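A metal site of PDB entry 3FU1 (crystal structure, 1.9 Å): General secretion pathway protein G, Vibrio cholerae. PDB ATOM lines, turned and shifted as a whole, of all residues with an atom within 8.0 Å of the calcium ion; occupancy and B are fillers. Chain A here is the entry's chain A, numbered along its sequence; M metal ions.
OD1 of Asp 105 is bound to the calcium ion (2.2 Å). O of Leu 91 is bound to the calcium ion (2.3 Å). The calcium ion is bound by O of Gly 103 (2.3 Å). The backbone carbonyl oxygen (O) of Gly 98 binds the calcium ion, 2.3 Å away. The calcium ion is bound by O of Gln 96. OD1 of Asp 94 binds the calcium ion.
Six residues have an atom within 4 Å of the calcium ion: Leu 91, Asp 94, Gln 96, Gly 98, Gly 103 and Asp 105. The nearest printed residue that does not touch the calcium ion is Glu 97 (4.2 Å).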
ATOM      1  N   THR A  90     -30.018   3.239  -6.758  1.00  0.00           N
ATOM      2  CA  THR A  90     -29.803   2.467  -7.958  1.00  0.00           C
ATOM      3  C   THR A  90     -28.952   1.247  -7.573  1.00  0.00           C
ATOM      4  O   THR A  90     -28.041   1.348  -6.742  1.00  0.00           O
ATOM      5  CB  THR A  90     -29.111   3.297  -9.073  1.00  0.00           C
ATOM      6  OG1 THR A  90     -28.703   2.435 -10.127  1.00  0.00           O
ATOM      7  CG2 THR A  90     -27.887   4.059  -8.578  1.00  0.00           C
ATOM      8  N   LEU A  91     -29.249   0.113  -8.188  1.00  0.00           N
ATOM      9  CA  LEU A  91     -28.472  -1.105  -7.989  1.00  0.00           C
ATOM     10  C   LEU A  91     -27.191  -1.144  -8.829  1.00  0.00           C
ATOM     11  O   LEU A  91     -26.453  -2.116  -8.764  1.00  0.00           O
ATOM     12  CB  LEU A  91     -29.351  -2.341  -8.253  1.00  0.00           C
ATOM     13  CG  LEU A  91     -30.561  -2.559  -7.326  1.00  0.00           C
ATOM     14  CD1 LEU A  91     -31.340  -3.811  -7.757  1.00  0.00           C
ATOM     15  CD2 LEU A  91     -30.141  -2.656  -5.873  1.00  0.00           C
ATOM     16  N   GLY A  92     -26.927  -0.107  -9.608  1.00  0.00           N
ATOM     17  CA  GLY A  92     -25.695  -0.017 -10.374  1.00  0.00           C
ATOM     18  C   GLY A  92     -25.694  -0.861 -11.637  1.00  0.00           C
ATOM     19  O   GLY A  92     -26.741  -1.323 -12.092  1.00  0.00           O
ATOM     20  N   ALA A  93     -24.497  -1.076 -12.178  1.00  0.00           N
ATOM     21  CA  ALA A  93     -24.346  -1.697 -13.496  1.00  0.00           C
ATOM     22  C   ALA A  93     -24.837  -3.143 -13.569  1.00  0.00           C
ATOM     23  O   ALA A  93     -25.260  -3.582 -14.637  1.00  0.00           O
ATOM     24  CB  ALA A  93     -22.904  -1.607 -13.952  1.00  0.00           C
ATOM     25  N   ASP A  94     -24.808  -3.875 -12.452  1.00  0.00           N
ATOM     26  CA  ASP A  94     -25.195  -5.280 -12.465  1.00  0.00           C
ATOM     27  C   ASP A  94     -26.708  -5.481 -12.280  1.00  0.00           C
ATOM     28  O   ASP A  94     -27.199  -6.594 -12.398  1.00  0.00           O
ATOM     29  CB  ASP A  94     -24.410  -6.090 -11.400  1.00  0.00           C
ATOM     30  CG  ASP A  94     -24.599  -5.561  -9.972  1.00  0.00           C
ATOM     31  OD1 ASP A  94     -25.446  -4.684  -9.784  1.00  0.00           O
ATOM     32  OD2 ASP A  94     -23.892  -6.037  -9.049  1.00  0.00           O
ATOM     33  N   GLY A  95     -27.433  -4.398 -11.980  1.00  0.00           N
ATOM     34  CA  GLY A  95     -28.881  -4.474 -11.765  1.00  0.00           C
ATOM     35  C   GLY A  95     -29.307  -5.422 -10.648  1.00  0.00           C
ATOM     36  O   GLY A  95     -30.447  -5.894 -10.640  1.00  0.00           O
ATOM     37  N   GLN A  96     -28.396  -5.687  -9.706  1.00  0.00           N
ATOM     38  CA  GLN A  96     -28.646  -6.617  -8.607  1.00  0.00           C
ATOM     39  C   GLN A  96     -28.125  -6.004  -7.315  1.00  0.00           C
ATOM     40  O   GLN A  96     -27.228  -5.153  -7.333  1.00  0.00           O
ATOM     41  CB  GLN A  96     -27.940  -7.956  -8.845  1.00  0.00           C
ATOM     42  CG  GLN A  96     -28.502  -8.802 -10.010  1.00  0.00           C
ATOM     43  CD  GLN A  96     -29.924  -9.328  -9.758  1.00  0.00           C
ATOM     44  OE1 GLN A  96     -30.408  -9.363  -8.614  1.00  0.00           O
ATOM     45  NE2 GLN A  96     -30.589  -9.745 -10.824  1.00  0.00           N
ATOM     46  N   GLU A  97     -28.697  -6.425  -6.194  1.00  0.00           N
ATOM     47  CA  GLU A  97     -28.275  -5.936  -4.884  1.00  0.00           C
ATOM     48  C   GLU A  97     -26.837  -6.332  -4.614  1.00  0.00           C
ATOM     49  O   GLU A  97     -26.406  -7.421  -4.964  1.00  0.00           O
ATOM     50  CB  GLU A  97     -29.175  -6.475  -3.782  1.00  0.00           C
ATOM     51  CG  GLU A  97     -30.573  -5.926  -3.822  1.00  0.00           C
ATOM     52  CD  GLU A  97     -31.417  -6.471  -2.690  1.00  0.00           C
ATOM     53  OE1 GLU A  97     -31.193  -6.057  -1.529  1.00  0.00           O
ATOM     54  OE2 GLU A  97     -32.308  -7.307  -2.962  1.00  0.00           O
ATOM     55  N   GLY A  98     -26.098  -5.446  -3.964  1.00  0.00           N
ATOM     56  CA  GLY A  98     -24.687  -5.685  -3.709  1.00  0.00           C
ATOM     57  C   GLY A  98     -23.821  -5.451  -4.928  1.00  0.00           C
ATOM     58  O   GLY A  98     -24.297  -5.012  -5.991  1.00  0.00           O
ATOM     59  N   GLY A  99     -22.544  -5.749  -4.763  1.00  0.00           N
ATOM     60  CA  GLY A  99     -21.570  -5.566  -5.821  1.00  0.00           C
ATOM     61  C   GLY A  99     -20.651  -4.405  -5.530  1.00  0.00           C
ATOM     62  O   GLY A  99     -20.804  -3.708  -4.522  1.00  0.00           O
ATOM     63  N   GLU A 100     -19.696  -4.211  -6.436  1.00  0.00           N
ATOM     64  CA  GLU A 100     -18.619  -3.263  -6.233  1.00  0.00           C
ATOM     65  C   GLU A 100     -18.178  -2.650  -7.565  1.00  0.00           C
ATOM     66  O   GLU A 100     -18.429  -3.219  -8.609  1.00  0.00           O
ATOM     67  CB  GLU A 100     -17.465  -4.000  -5.553  1.00  0.00           C
ATOM     68  CG  GLU A 100     -16.482  -3.111  -4.862  1.00  0.00           C
ATOM     69  CD  GLU A 100     -15.405  -3.858  -4.124  1.00  0.00           C
ATOM     70  OE1 GLU A 100     -15.648  -4.993  -3.617  1.00  0.00           O
ATOM     71  OE2 GLU A 100     -14.292  -3.308  -4.034  1.00  0.00           O
ATOM     72  N   GLY A 101     -17.527  -1.491  -7.513  1.00  0.00           N
ATOM     73  CA  GLY A 101     -17.117  -0.798  -8.733  1.00  0.00           C
ATOM     74  C   GLY A 101     -18.360  -0.296  -9.463  1.00  0.00           C
ATOM     75  O   GLY A 101     -19.271   0.224  -8.845  1.00  0.00           O
ATOM     76  N   THR A 102     -18.428  -0.501 -10.782  1.00  0.00           N
ATOM     77  CA  THR A 102     -19.626  -0.058 -11.508  1.00  0.00           C
ATOM     78  C   THR A 102     -20.898  -0.734 -11.000  1.00  0.00           C
ATOM     79  O   THR A 102     -21.981  -0.166 -11.099  1.00  0.00           O
ATOM     80  CB  THR A 102     -19.503  -0.259 -13.027  1.00  0.00           C
ATOM     81  OG1 THR A 102     -19.401  -1.662 -13.323  1.00  0.00           O
ATOM     82  CG2 THR A 102     -18.262   0.471 -13.555  1.00  0.00           C
ATOM     83  N   GLY A 103     -20.770  -1.950 -10.453  1.00  0.00           N
ATOM     84  CA  GLY A 103     -21.902  -2.662  -9.866  1.00  0.00           C
ATOM     85  C   GLY A 103     -22.316  -2.229  -8.463  1.00  0.00           C
ATOM     86  O   GLY A 103     -23.294  -2.750  -7.932  1.00  0.00           O
ATOM     87  N   ALA A 104     -21.594  -1.276  -7.884  1.00  0.00           N
ATOM     88  CA  ALA A 104     -21.883  -0.770  -6.541  1.00  0.00           C
ATOM     89  C   ALA A 104     -23.287  -0.144  -6.459  1.00  0.00           C
ATOM     90  O   ALA A 104     -23.678   0.652  -7.321  1.00  0.00           O
ATOM     91  CB  ALA A 104     -20.842   0.259  -6.136  1.00  0.00           C
ATOM     92  N   ASP A 105     -24.025  -0.525  -5.427  1.00  0.00           N
ATOM     93  CA  ASP A 105     -25.326   0.083  -5.161  1.00  0.00           C
ATOM     94  C   ASP A 105     -25.092   1.486  -4.624  1.00  0.00           C
ATOM     95  O   ASP A 105     -24.298   1.648  -3.709  1.00  0.00           O
ATOM     96  CB  ASP A 105     -26.117  -0.740  -4.144  1.00  0.00           C
ATOM     97  CG  ASP A 105     -26.412  -2.145  -4.619  1.00  0.00           C
ATOM     98  OD1 ASP A 105     -26.182  -2.460  -5.820  1.00  0.00           O
ATOM     99  OD2 ASP A 105     -26.858  -2.959  -3.785  1.00  0.00           O
ATOM    100  N   ILE A 106     -25.735   2.470  -5.221  1.00  0.00           N
ATOM    101  CA  ILE A 106     -25.644   3.864  -4.793  1.00  0.00           C
ATOM    102  C   ILE A 106     -27.011   4.281  -4.258  1.00  0.00           C
ATOM    103  O   ILE A 106     -28.005   4.219  -4.973  1.00  0.00           O
ATOM    104  CB  ILE A 106     -25.160   4.797  -5.947  1.00  0.00           C
ATOM    105  CG1 ILE A 106     -23.812   4.289  -6.504  1.00  0.00           C
ATOM    106  CG2 ILE A 106     -25.056   6.258  -5.452  1.00  0.00           C
ATOM    107  CD1 ILE A 106     -23.310   5.045  -7.748  1.00  0.00           C
HETATM  108 CA    CA M   1     -25.370  -3.665  -7.536  1.00  0.00          CA
